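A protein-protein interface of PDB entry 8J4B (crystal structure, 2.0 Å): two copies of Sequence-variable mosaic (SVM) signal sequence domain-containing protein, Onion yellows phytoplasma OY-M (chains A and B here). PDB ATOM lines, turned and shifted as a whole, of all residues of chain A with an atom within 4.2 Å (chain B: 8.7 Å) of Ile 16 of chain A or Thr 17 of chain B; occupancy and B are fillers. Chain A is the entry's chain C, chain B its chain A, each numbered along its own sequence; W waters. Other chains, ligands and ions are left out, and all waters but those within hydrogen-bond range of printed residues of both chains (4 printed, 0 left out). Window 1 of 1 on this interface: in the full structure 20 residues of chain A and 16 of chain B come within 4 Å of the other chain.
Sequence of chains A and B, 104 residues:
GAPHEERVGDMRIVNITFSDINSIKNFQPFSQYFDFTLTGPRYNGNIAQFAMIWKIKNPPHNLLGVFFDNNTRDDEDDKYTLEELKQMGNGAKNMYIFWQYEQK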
ATOM      1  N   HIS A   4      24.582 -32.935  -0.764  1.00  0.00           N
ATOM      2  CA  HIS A   4      25.896 -32.539  -0.280  1.00  0.00           C
ATOM      3  C   HIS A   4      25.991 -31.061   0.068  1.00  0.00           C
ATOM      4  O   HIS A   4      27.064 -30.610   0.487  1.00  0.00           O
ATOM      5  CB  HIS A   4      26.950 -32.843  -1.342  1.00  0.00           C
ATOM      6  CG  HIS A   4      26.666 -32.163  -2.641  1.00  0.00           C
ATOM      7  ND1 HIS A   4      25.670 -32.587  -3.495  1.00  0.00           N
ATOM      8  CD2 HIS A   4      27.196 -31.050  -3.201  1.00  0.00           C
ATOM      9  CE1 HIS A   4      25.622 -31.783  -4.543  1.00  0.00           C
ATOM     10  NE2 HIS A   4      26.532 -30.839  -4.385  1.00  0.00           N
ATOM     11  N   VAL A  14      25.129 -22.656  -2.213  1.00  0.00           N
ATOM     12  CA  VAL A  14      25.026 -23.254  -3.544  1.00  0.00           C
ATOM     13  C   VAL A  14      26.266 -22.847  -4.337  1.00  0.00           C
ATOM     14  O   VAL A  14      26.425 -21.671  -4.686  1.00  0.00           O
ATOM     15  CB  VAL A  14      23.742 -22.802  -4.257  1.00  0.00           C
ATOM     16  CG1 VAL A  14      23.533 -23.579  -5.575  1.00  0.00           C
ATOM     17  CG2 VAL A  14      22.534 -22.968  -3.331  1.00  0.00           C
ATOM     18  N   ASN A  15      27.162 -23.805  -4.621  1.00  0.00           N
ATOM     19  CA  ASN A  15      28.366 -23.549  -5.415  1.00  0.00           C
ATOM     20  C   ASN A  15      28.076 -23.966  -6.849  1.00  0.00           C
ATOM     21  O   ASN A  15      27.891 -25.154  -7.123  1.00  0.00           O
ATOM     22  CB  ASN A  15      29.577 -24.316  -4.874  1.00  0.00           C
ATOM     23  CG  ASN A  15      29.949 -23.896  -3.459  1.00  0.00           C
ATOM     24  OD1 ASN A  15      30.488 -22.806  -3.243  1.00  0.00           O
ATOM     25  ND2 ASN A  15      29.639 -24.756  -2.486  1.00  0.00           N
ATOM     26  N   ILE A  16      28.047 -22.996  -7.762  1.00  0.00           N
ATOM     27  CA  ILE A  16      27.767 -23.239  -9.173  1.00  0.00           C
ATOM     28  C   ILE A  16      29.049 -22.967  -9.952  1.00  0.00           C
ATOM     29  O   ILE A  16      29.728 -21.964  -9.703  1.00  0.00           O
ATOM     30  CB  ILE A  16      26.617 -22.344  -9.682  1.00  0.00           C
ATOM     31  CG1 ILE A  16      25.409 -22.397  -8.736  1.00  0.00           C
ATOM     32  CG2 ILE A  16      26.188 -22.747 -11.070  1.00  0.00           C
ATOM     33  CD1 ILE A  16      24.160 -21.730  -9.325  1.00  0.00           C
ATOM     34  N   THR A  17      29.370 -23.835 -10.906  1.00  0.00           N
ATOM     35  CA  THR A  17      30.636 -23.766 -11.628  1.00  0.00           C
ATOM     36  C   THR A  17      30.380 -23.464 -13.103  1.00  0.00           C
ATOM     37  O   THR A  17      29.413 -23.965 -13.684  1.00  0.00           O
ATOM     38  CB  THR A  17      31.412 -25.083 -11.457  1.00  0.00           C
ATOM     39  OG1 THR A  17      31.694 -25.314 -10.062  1.00  0.00           O
ATOM     40  CG2 THR A  17      32.732 -25.066 -12.236  1.00  0.00           C
ATOM     41  N   PHE A  18      31.255 -22.649 -13.706  1.00  0.00           N
ATOM     42  CA  PHE A  18      31.128 -22.219 -15.090  1.00  0.00           C
ATOM     43  C   PHE A  18      32.450 -22.431 -15.822  1.00  0.00           C
ATOM     44  O   PHE A  18      33.521 -22.540 -15.209  1.00  0.00           O
ATOM     45  CB  PHE A  18      30.699 -20.743 -15.188  1.00  0.00           C
ATOM     46  CG  PHE A  18      29.416 -20.444 -14.457  1.00  0.00           C
ATOM     47  CD1 PHE A  18      29.417 -20.256 -13.086  1.00  0.00           C
ATOM     48  CD2 PHE A  18      28.209 -20.414 -15.132  1.00  0.00           C
ATOM     49  CE1 PHE A  18      28.238 -20.010 -12.405  1.00  0.00           C
ATOM     50  CE2 PHE A  18      27.023 -20.166 -14.461  1.00  0.00           C
ATOM     51  CZ  PHE A  18      27.042 -19.975 -13.090  1.00  0.00           C
ATOM     52  N   PHE A  27      23.239 -16.424 -17.725  1.00  0.00           N
ATOM     53  CA  PHE A  27      22.621 -17.198 -16.646  1.00  0.00           C
ATOM     54  C   PHE A  27      21.542 -16.360 -15.965  1.00  0.00           C
ATOM     55  O   PHE A  27      21.808 -15.649 -14.993  1.00  0.00           O
ATOM     56  CB  PHE A  27      23.690 -17.666 -15.658  1.00  0.00           C
ATOM     57  CG  PHE A  27      23.165 -18.560 -14.561  1.00  0.00           C
ATOM     58  CD1 PHE A  27      21.991 -19.287 -14.724  1.00  0.00           C
ATOM     59  CD2 PHE A  27      23.865 -18.686 -13.370  1.00  0.00           C
ATOM     60  CE1 PHE A  27      21.513 -20.112 -13.709  1.00  0.00           C
ATOM     61  CE2 PHE A  27      23.390 -19.509 -12.344  1.00  0.00           C
ATOM     62  CZ  PHE A  27      22.218 -20.224 -12.522  1.00  0.00           C
ATOM     63  N   ILE A  97      27.346 -19.072  -4.845  1.00  0.00           N
ATOM     64  CA  ILE A  97      28.767 -18.828  -5.005  1.00  0.00           C
ATOM     65  C   ILE A  97      29.153 -19.320  -6.387  1.00  0.00           C
ATOM     66  O   ILE A  97      28.963 -20.504  -6.701  1.00  0.00           O
ATOM     67  CB  ILE A  97      29.588 -19.532  -3.913  1.00  0.00           C
ATOM     68  CG1 ILE A  97      29.100 -19.130  -2.524  1.00  0.00           C
ATOM     69  CG2 ILE A  97      31.037 -19.183  -4.044  1.00  0.00           C
ATOM     70  CD1 ILE A  97      29.898 -19.827  -1.409  1.00  0.00           C
ATOM     71  N   PHE A  98      29.703 -18.424  -7.204  1.00  0.00           N
ATOM     72  CA  PHE A  98      29.972 -18.713  -8.606  1.00  0.00           C
ATOM     73  C   PHE A  98      31.459 -18.964  -8.790  1.00  0.00           C
ATOM     74  O   PHE A  98      32.282 -18.161  -8.335  1.00  0.00           O
ATOM     75  CB  PHE A  98      29.499 -17.556  -9.493  1.00  0.00           C
ATOM     76  CG  PHE A  98      28.043 -17.187  -9.291  1.00  0.00           C
ATOM     77  CD1 PHE A  98      27.667 -16.328  -8.276  1.00  0.00           C
ATOM     78  CD2 PHE A  98      27.052 -17.712 -10.110  1.00  0.00           C
ATOM     79  CE1 PHE A  98      26.318 -15.983  -8.083  1.00  0.00           C
ATOM     80  CE2 PHE A  98      25.713 -17.380  -9.917  1.00  0.00           C
ATOM     81  CZ  PHE A  98      25.348 -16.511  -8.902  1.00  0.00           C
ATOM     82  N   TRP A  99      31.804 -20.080  -9.458  1.00  0.00           N
ATOM     83  CA  TRP A  99      33.188 -20.523  -9.599  1.00  0.00           C
ATOM     84  C   TRP A  99      33.568 -20.755 -11.061  1.00  0.00           C
ATOM     85  O   TRP A  99      32.753 -21.211 -11.874  1.00  0.00           O
ATOM     86  CB  TRP A  99      33.443 -21.835  -8.857  1.00  0.00           C
ATOM     87  CG  TRP A  99      33.186 -21.791  -7.381  1.00  0.00           C
ATOM     88  CD1 TRP A  99      32.026 -22.097  -6.735  1.00  0.00           C
ATOM     89  CD2 TRP A  99      34.135 -21.436  -6.364  1.00  0.00           C
ATOM     90  NE1 TRP A  99      32.197 -21.961  -5.368  1.00  0.00           N
ATOM     91  CE2 TRP A  99      33.489 -21.566  -5.123  1.00  0.00           C
ATOM     92  CE3 TRP A  99      35.478 -21.036  -6.392  1.00  0.00           C
ATOM     93  CZ2 TRP A  99      34.133 -21.288  -3.912  1.00  0.00           C
ATOM     94  CZ3 TRP A  99      36.120 -20.769  -5.189  1.00  0.00           C
ATOM     95  CH2 TRP A  99      35.441 -20.897  -3.965  1.00  0.00           C
ATOM     96  N   VAL B  14      34.013 -35.454  -6.262  1.00  0.00           N
ATOM     97  CA  VAL B  14      33.906 -34.056  -6.672  1.00  0.00           C
ATOM     98  C   VAL B  14      32.480 -33.811  -7.151  1.00  0.00           C
ATOM     99  O   VAL B  14      32.101 -34.219  -8.256  1.00  0.00           O
ATOM    100  CB  VAL B  14      34.920 -33.697  -7.762  1.00  0.00           C
ATOM    101  CG1 VAL B  14      34.873 -32.198  -8.054  1.00  0.00           C
ATOM    102  CG2 VAL B  14      36.306 -34.126  -7.344  1.00  0.00           C
ATOM    103  N   ASN B  15      31.678 -33.148  -6.331  1.00  0.00           N
ATOM    104  CA  ASN B  15      30.370 -32.710  -6.781  1.00  0.00           C
ATOM    105  C   ASN B  15      30.530 -31.399  -7.536  1.00  0.00           C
ATOM    106  O   ASN B  15      31.144 -30.458  -7.022  1.00  0.00           O
ATOM    107  CB  ASN B  15      29.423 -32.545  -5.587  1.00  0.00           C
ATOM    108  CG  ASN B  15      29.121 -33.866  -4.904  1.00  0.00           C
ATOM    109  OD1 ASN B  15      28.451 -34.728  -5.463  1.00  0.00           O
ATOM    110  ND2 ASN B  15      29.615 -34.029  -3.692  1.00  0.00           N
ATOM    111  N   ILE B  16      30.011 -31.342  -8.759  1.00  0.00           N
ATOM    112  CA  ILE B  16      30.004 -30.118  -9.558  1.00  0.00           C
ATOM    113  C   ILE B  16      28.563 -29.785  -9.920  1.00  0.00           C
ATOM    114  O   ILE B  16      27.857 -30.628 -10.478  1.00  0.00           O
ATOM    115  CB  ILE B  16      30.848 -30.259 -10.835  1.00  0.00           C
ATOM    116  CG1 ILE B  16      32.277 -30.667 -10.490  1.00  0.00           C
ATOM    117  CG2 ILE B  16      30.859 -28.954 -11.616  1.00  0.00           C
ATOM    118  CD1 ILE B  16      33.171 -30.806 -11.721  1.00  0.00           C
ATOM    119  N   THR B  17      28.136 -28.557  -9.618  1.00  0.00           N
ATOM    120  CA  THR B  17      26.797 -28.081  -9.939  1.00  0.00           C
ATOM    121  C   THR B  17      26.844 -27.097 -11.102  1.00  0.00           C
ATOM    122  O   THR B  17      27.670 -26.178 -11.115  1.00  0.00           O
ATOM    123  CB  THR B  17      26.150 -27.402  -8.729  1.00  0.00           C
ATOM    124  OG1 THR B  17      26.176 -28.296  -7.612  1.00  0.00           O
ATOM    125  CG2 THR B  17      24.717 -27.060  -9.044  1.00  0.00           C
ATOM    126  N   PHE B  18      25.928 -27.264 -12.053  1.00  0.00           N
ATOM    127  CA  PHE B  18      25.894 -26.476 -13.277  1.00  0.00           C
ATOM    128  C   PHE B  18      24.634 -25.625 -13.351  1.00  0.00           C
ATOM    129  O   PHE B  18      23.606 -25.945 -12.753  1.00  0.00           O
ATOM    130  CB  PHE B  18      25.937 -27.370 -14.522  1.00  0.00           C
ATOM    131  CG  PHE B  18      27.170 -28.190 -14.622  1.00  0.00           C
ATOM    132  CD1 PHE B  18      28.313 -27.676 -15.207  1.00  0.00           C
ATOM    133  CD2 PHE B  18      27.188 -29.478 -14.130  1.00  0.00           C
ATOM    134  CE1 PHE B  18      29.462 -28.432 -15.290  1.00  0.00           C
ATOM    135  CE2 PHE B  18      28.337 -30.252 -14.216  1.00  0.00           C
ATOM    136  CZ  PHE B  18      29.476 -29.727 -14.793  1.00  0.00           C
ATOM    137  N   SER B  19      24.709 -24.558 -14.144  1.00  0.00           N
ATOM    138  CA  SER B  19      23.528 -23.730 -14.369  1.00  0.00           C
ATOM    139  C   SER B  19      22.458 -24.493 -15.149  1.00  0.00           C
ATOM    140  O   SER B  19      21.262 -24.365 -14.862  1.00  0.00           O
ATOM    141  CB  SER B  19      23.909 -22.440 -15.106  1.00  0.00           C
ATOM    142  OG  SER B  19      24.588 -22.704 -16.317  1.00  0.00           O
ATOM    143  N   ASP B  20      22.868 -25.278 -16.146  1.00  0.00           N
ATOM    144  CA  ASP B  20      21.958 -26.092 -16.944  1.00  0.00           C
ATOM    145  C   ASP B  20      22.772 -27.206 -17.589  1.00  0.00           C
ATOM    146  O   ASP B  20      24.002 -27.227 -17.513  1.00  0.00           O
ATOM    147  CB  ASP B  20      21.220 -25.266 -18.003  1.00  0.00           C
ATOM    148  CG  ASP B  20      22.160 -24.412 -18.855  1.00  0.00           C
ATOM    149  OD1 ASP B  20      23.291 -24.850 -19.174  1.00  0.00           O
ATOM    150  OD2 ASP B  20      21.760 -23.283 -19.212  1.00  0.00           O
ATOM    151  N   ILE B  21      22.072 -28.141 -18.229  1.00  0.00           N
ATOM    152  CA  ILE B  21      22.785 -29.274 -18.801  1.00  0.00           C
ATOM    153  C   ILE B  21      23.568 -28.843 -20.039  1.00  0.00           C
ATOM    154  O   ILE B  21      24.695 -29.297 -20.261  1.00  0.00           O
ATOM    155  CB  ILE B  21      21.822 -30.436 -19.095  1.00  0.00           C
ATOM    156  CG1 ILE B  21      22.599 -31.602 -19.711  1.00  0.00           C
ATOM    157  CG2 ILE B  21      20.687 -29.981 -19.997  1.00  0.00           C
ATOM    158  CD1 ILE B  21      22.086 -32.979 -19.296  1.00  0.00           C
ATOM    159  N   SER B  23      25.285 -26.384 -20.440  1.00  0.00           N
ATOM    160  CA  SER B  23      26.570 -25.797 -20.061  1.00  0.00           C
ATOM    161  C   SER B  23      27.691 -26.825 -20.071  1.00  0.00           C
ATOM    162  O   SER B  23      28.852 -26.481 -20.311  1.00  0.00           O
ATOM    163  CB  SER B  23      26.484 -25.169 -18.667  1.00  0.00           C
ATOM    164  OG  SER B  23      25.554 -24.101 -18.670  1.00  0.00           O
ATOM    165  N   ILE B  24      27.373 -28.083 -19.767  1.00  0.00           N
ATOM    166  CA  ILE B  24      28.396 -29.117 -19.714  1.00  0.00           C
ATOM    167  C   ILE B  24      29.128 -29.263 -21.045  1.00  0.00           C
ATOM    168  O   ILE B  24      30.266 -29.743 -21.076  1.00  0.00           O
ATOM    169  CB  ILE B  24      27.751 -30.442 -19.270  1.00  0.00           C
ATOM    170  CG1 ILE B  24      27.051 -30.264 -17.916  1.00  0.00           C
ATOM    171  CG2 ILE B  24      28.781 -31.546 -19.179  1.00  0.00           C
ATOM    172  CD1 ILE B  24      26.245 -31.453 -17.495  1.00  0.00           C
ATOM    173  N   PHE B  27      32.502 -27.831 -21.126  1.00  0.00           N
ATOM    174  CA  PHE B  27      33.419 -28.291 -20.095  1.00  0.00           C
ATOM    175  C   PHE B  27      34.328 -29.355 -20.671  1.00  0.00           C
ATOM    176  O   PHE B  27      33.887 -30.479 -20.922  1.00  0.00           O
ATOM    177  CB  PHE B  27      32.665 -28.853 -18.895  1.00  0.00           C
ATOM    178  CG  PHE B  27      32.357 -27.839 -17.864  1.00  0.00           C
ATOM    179  CD1 PHE B  27      31.404 -26.868 -18.108  1.00  0.00           C
ATOM    180  CD2 PHE B  27      33.015 -27.852 -16.644  1.00  0.00           C
ATOM    181  CE1 PHE B  27      31.103 -25.922 -17.154  1.00  0.00           C
ATOM    182  CE2 PHE B  27      32.720 -26.912 -15.689  1.00  0.00           C
ATOM    183  CZ  PHE B  27      31.760 -25.941 -15.948  1.00  0.00           C
ATOM    184  N   ASN B  62      17.804 -34.141  -9.692  1.00  0.00           N
ATOM    185  CA  ASN B  62      18.771 -33.204 -10.258  1.00  0.00           C
ATOM    186  C   ASN B  62      20.151 -33.807 -10.519  1.00  0.00           C
ATOM    187  O   ASN B  62      21.060 -33.079 -10.963  1.00  0.00           O
ATOM    188  CB  ASN B  62      18.930 -31.949  -9.390  1.00  0.00           C
ATOM    189  CG  ASN B  62      17.813 -30.953  -9.623  1.00  0.00           C
ATOM    190  OD1 ASN B  62      17.342 -30.790 -10.750  1.00  0.00           O
ATOM    191  ND2 ASN B  62      17.373 -30.301  -8.560  1.00  0.00           N
ATOM    192  N   LEU B  64      22.793 -35.344 -12.773  1.00  0.00           N
ATOM    193  CA  LEU B  64      22.950 -35.369 -14.223  1.00  0.00           C
ATOM    194  C   LEU B  64      23.883 -36.457 -14.740  1.00  0.00           C
ATOM    195  O   LEU B  64      23.762 -36.843 -15.910  1.00  0.00           O
ATOM    196  CB  LEU B  64      23.473 -34.020 -14.732  1.00  0.00           C
ATOM    197  CG  LEU B  64      22.578 -32.803 -14.485  1.00  0.00           C
ATOM    198  CD1 LEU B  64      23.258 -31.556 -15.039  1.00  0.00           C
ATOM    199  CD2 LEU B  64      21.199 -33.015 -15.111  1.00  0.00           C
ATOM    200  N   ILE B  97      30.661 -35.954  -9.898  1.00  0.00           N
ATOM    201  CA  ILE B  97      29.217 -36.119  -9.800  1.00  0.00           C
ATOM    202  C   ILE B  97      28.580 -34.805 -10.240  1.00  0.00           C
ATOM    203  O   ILE B  97      28.804 -33.764  -9.608  1.00  0.00           O
ATOM    204  CB  ILE B  97      28.800 -36.522  -8.376  1.00  0.00           C
ATOM    205  CG1 ILE B  97      29.603 -37.746  -7.913  1.00  0.00           C
ATOM    206  CG2 ILE B  97      27.305 -36.824  -8.296  1.00  0.00           C
ATOM    207  CD1 ILE B  97      29.157 -38.305  -6.559  1.00  0.00           C
ATOM    208  N   PHE B  98      27.813 -34.844 -11.335  1.00  0.00           N
ATOM    209  CA  PHE B  98      27.280 -33.634 -11.963  1.00  0.00           C
ATOM    210  C   PHE B  98      25.844 -33.407 -11.528  1.00  0.00           C
ATOM    211  O   PHE B  98      25.030 -34.336 -11.577  1.00  0.00           O
ATOM    212  CB  PHE B  98      27.331 -33.729 -13.489  1.00  0.00           C
ATOM    213  CG  PHE B  98      28.687 -34.081 -14.019  1.00  0.00           C
ATOM    214  CD1 PHE B  98      29.772 -33.265 -13.779  1.00  0.00           C
ATOM    215  CD2 PHE B  98      28.881 -35.241 -14.744  1.00  0.00           C
ATOM    216  CE1 PHE B  98      31.031 -33.596 -14.253  1.00  0.00           C
ATOM    217  CE2 PHE B  98      30.135 -35.577 -15.212  1.00  0.00           C
ATOM    218  CZ  PHE B  98      31.210 -34.747 -14.968  1.00  0.00           C
ATOM    219  N   TRP B  99      25.527 -32.159 -11.160  1.00  0.00           N
ATOM    220  CA  TRP B  99      24.221 -31.793 -10.621  1.00  0.00           C
ATOM    221  C   TRP B  99      23.646 -30.580 -11.347  1.00  0.00           C
ATOM    222  O   TRP B  99      24.376 -29.670 -11.745  1.00  0.00           O
ATOM    223  CB  TRP B  99      24.298 -31.449  -9.117  1.00  0.00           C
ATOM    224  CG  TRP B  99      24.763 -32.566  -8.244  1.00  0.00           C
ATOM    225  CD1 TRP B  99      26.038 -32.835  -7.870  1.00  0.00           C
ATOM    226  CD2 TRP B  99      23.937 -33.544  -7.614  1.00  0.00           C
ATOM    227  NE1 TRP B  99      26.068 -33.940  -7.052  1.00  0.00           N
ATOM    228  CE2 TRP B  99      24.785 -34.397  -6.882  1.00  0.00           C
ATOM    229  CE3 TRP B  99      22.556 -33.795  -7.614  1.00  0.00           C
ATOM    230  CZ2 TRP B  99      24.300 -35.480  -6.139  1.00  0.00           C
ATOM    231  CZ3 TRP B  99      22.071 -34.874  -6.871  1.00  0.00           C
ATOM    232  CH2 TRP B  99      22.947 -35.704  -6.145  1.00  0.00           C
ATOM    233  N   GLN B 100      22.323 -30.562 -11.466  1.00  0.00           N
ATOM    234  CA  GLN B 100      21.573 -29.395 -11.929  1.00  0.00           C
ATOM    235  C   GLN B 100      21.277 -28.496 -10.727  1.00  0.00           C
ATOM    236  O   GLN B 100      20.692 -28.962  -9.743  1.00  0.00           O
ATOM    237  CB  GLN B 100      20.279 -29.864 -12.595  1.00  0.00           C
ATOM    238  CG  GLN B 100      19.251 -28.798 -12.816  1.00  0.00           C
ATOM    239  CD  GLN B 100      19.703 -27.801 -13.866  1.00  0.00           C
ATOM    240  OE1 GLN B 100      19.917 -28.149 -15.036  1.00  0.00           O
ATOM    241  NE2 GLN B 100      19.870 -26.550 -13.448  1.00  0.00           N
ATOM    242  N   TYR B 101      21.698 -27.225 -10.777  1.00  0.00           N
ATOM    243  CA  TYR B 101      21.412 -26.358  -9.635  1.00  0.00           C
ATOM    244  C   TYR B 101      19.906 -26.140  -9.517  1.00  0.00           C
ATOM    245  O   TYR B 101      19.164 -26.251 -10.497  1.00  0.00           O
ATOM    246  CB  TYR B 101      22.114 -25.008  -9.771  1.00  0.00           C
ATOM    247  CG  TYR B 101      21.229 -23.945 -10.363  1.00  0.00           C
ATOM    248  CD1 TYR B 101      20.920 -23.951 -11.717  1.00  0.00           C
ATOM    249  CD2 TYR B 101      20.678 -22.950  -9.563  1.00  0.00           C
ATOM    250  CE1 TYR B 101      20.096 -22.982 -12.258  1.00  0.00           C
ATOM    251  CE2 TYR B 101      19.859 -21.977 -10.094  1.00  0.00           C
ATOM    252  CZ  TYR B 101      19.568 -21.997 -11.435  1.00  0.00           C
ATOM    253  OH  TYR B 101      18.744 -21.002 -11.914  1.00  0.00           O
ATOM    254  N   GLU B 102      19.455 -25.820  -8.302  1.00  0.00           N
ATOM    255  CA  GLU B 102      18.063 -25.428  -8.084  1.00  0.00           C
ATOM    256  C   GLU B 102      17.980 -24.302  -7.052  1.00  0.00           C
ATOM    257  O   GLU B 102      18.884 -24.101  -6.231  1.00  0.00           O
ATOM    258  CB  GLU B 102      17.196 -26.619  -7.642  1.00  0.00           C
ATOM    259  CG  GLU B 102      17.705 -27.352  -6.419  1.00  0.00           C
ATOM    260  CD  GLU B 102      16.684 -28.356  -5.870  1.00  0.00           C
ATOM    261  OE1 GLU B 102      15.488 -28.232  -6.228  1.00  0.00           O
ATOM    262  OE2 GLU B 102      17.073 -29.258  -5.082  1.00  0.00           O
ATOM    263  N   GLN B 103      16.874 -23.558  -7.111  1.00  0.00           N
ATOM    264  CA  GLN B 103      16.658 -22.412  -6.231  1.00  0.00           C
ATOM    265  C   GLN B 103      16.014 -22.795  -4.903  1.00  0.00           C
ATOM    266  O   GLN B 103      15.700 -21.907  -4.109  1.00  0.00           O
ATOM    267  CB  GLN B 103      15.818 -21.355  -6.962  1.00  0.00           C
ATOM    268  CG  GLN B 103      16.517 -20.836  -8.233  1.00  0.00           C
ATOM    269  CD  GLN B 103      15.720 -19.772  -8.955  1.00  0.00           C
ATOM    270  OE1 GLN B 103      14.786 -19.207  -8.394  1.00  0.00           O
ATOM    271  NE2 GLN B 103      16.088 -19.489 -10.204  1.00  0.00           N
HETATM  272  O   HOH W   1      26.191 -26.580  -4.848  1.00  0.00           O
HETATM  273  O   HOH W   2      29.763 -26.459  -8.400  1.00  0.00           O
HETATM  274  O   HOH W   3      28.298 -28.961  -5.795  1.00  0.00           O
HETATM  275  O   HOH W   4      27.201 -23.988 -15.354  1.00  0.00           O
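O of Thr 17 of chain B is in hydrogen-bond range of N of Thr 17 of chain A, 2.9 Å away.
Water W2 lies within hydrogen-bond range of the backbone carbonyl oxygen of Asn 15 of chain A, the side-chain hydroxyl of Thr 17 of chain A and the backbone NH of Thr 17 of chain B.
Water W4 bridges O of Thr 17 of chain A (2.8 Å) and N of Ser 19 of chain B (2.8 Å).
Water W3 lies within hydrogen-bond range of the side-chain hydroxyl of Thr 17 of chain B (2.9 Å), a ring nitrogen (NE2) of His 4 of chain A (2.9 Å) and the backbone carbonyl oxygen of Asn 15 of chain B (3.4 Å).
Water W1 bridges N of Asn 15 of chain A (2.9 Å) and OG1 of Thr 17 of chain B (3.3 Å).
The backbone carbonyl oxygen of Ile 16 of chain A is in hydrogen-bond range of the backbone NH of Trp 99 of chain A.
N of Phe 18 of chain B is in hydrogen-bond range of O of Trp 99 of chain B (2.9 Å).
O of Ile 97 of chain B is in hydrogen-bond range of N of Ile 16 of chain B (2.8 Å).
The backbone carbonyl oxygen (O) of Ile 16 of chain B lies within hydrogen-bond range of the backbone NH (N) of Trp 99 of chain B, 2.9 Å away.
O of Phe 18 of chain B sits at hydrogen-bond distance from N of Tyr 101 of chain B (3.0 Å).
The backbone carbonyl oxygen of Ile 97 of chain A sits at hydrogen-bond distance from the backbone NH of Ile 16 of chain A.
Of the printed residues of chain B, Ile 16 of chain A touches Thr 17 (3.5 Å), Phe 18 (3.99 Å), Ser 19 (3.9 Å) and Tyr 101 (3.7 Å).
Printed residues of chain A within 4 Å of Thr 17 of chain B: Asn 15 (3.3 Å), Ile 16 (3.5 Å) and Thr 17 (2.9 Å).
Of the printed residues of chain A, Asn 15 of chain B touches His 4.
Of the printed residues of chain B, His 4 of chain A touches Asn 15 (3.6 Å) and Trp 99 (3.3 Å).
Asp 20 of chain B touches none of the printed residues of chain A.
Phe 98 of chain A touches none of the printed residues of chain B.
The nearest printed residue of chain A that does not touch Asn 15 of chain B is Thr 17 of chain A (6.0 Å).
Of the 20 printed residues of chain B, 8 touch a printed residue of chain A.
Hydrophobic or aromatic side chains of chain B that line the printed part of chain A: Ile 16, Phe 27, Trp 99 and Tyr 101.
Among the printed residues, 14 pairs touch across the chains.
Among the printed residues, merely in contact across the chains: Asn 15 of chain A with Thr 17 of chain B, His 4 of chain A with Trp 99 of chain B, Phe 27 of chain A with Tyr 101 of chain B, Ile 16 of chain A with Thr 17 of chain B, His 4 of chain A with Asn 15 of chain B, Phe 18 of chain A with Phe 27 of chain B, Phe 27 of chain A with Ser 19 of chain B, Ile 16 of chain A with Tyr 101 of chain B, Thr 17 of chain A with Phe 27 of chain B, Ile 16 of chain A with Ser 19 of chain B, Phe 18 of chain A with Ser 19 of chain B, Thr 17 of chain A with Ile 16 of chain B and Ile 16 of chain A with Phe 18 of chain B.
Asn 15 of chain A touches Thr 17 of chain B, but with the chains exchanged Thr 17 of chain A does not touch Asn 15 of chain B (6.0 Å).
Ile 16 of chain A touches Phe 18 of chain B, but with the chains exchanged Phe 18 of chain A does not touch Ile 16 of chain B (6.7 Å).
Thr 17 of chain A touches Phe 27 of chain B, but with the chains exchanged Phe 27 of chain A does not touch Thr 17 of chain B (8.0 Å).
Phe 18 of chain A touches Phe 27 of chain B, but with the chains exchanged Phe 27 of chain A does not touch Phe 18 of chain B (5.9 Å).
Positions printed for both chains: 14, 15, 16, 17, 18, 27, 97, 98 and 99.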
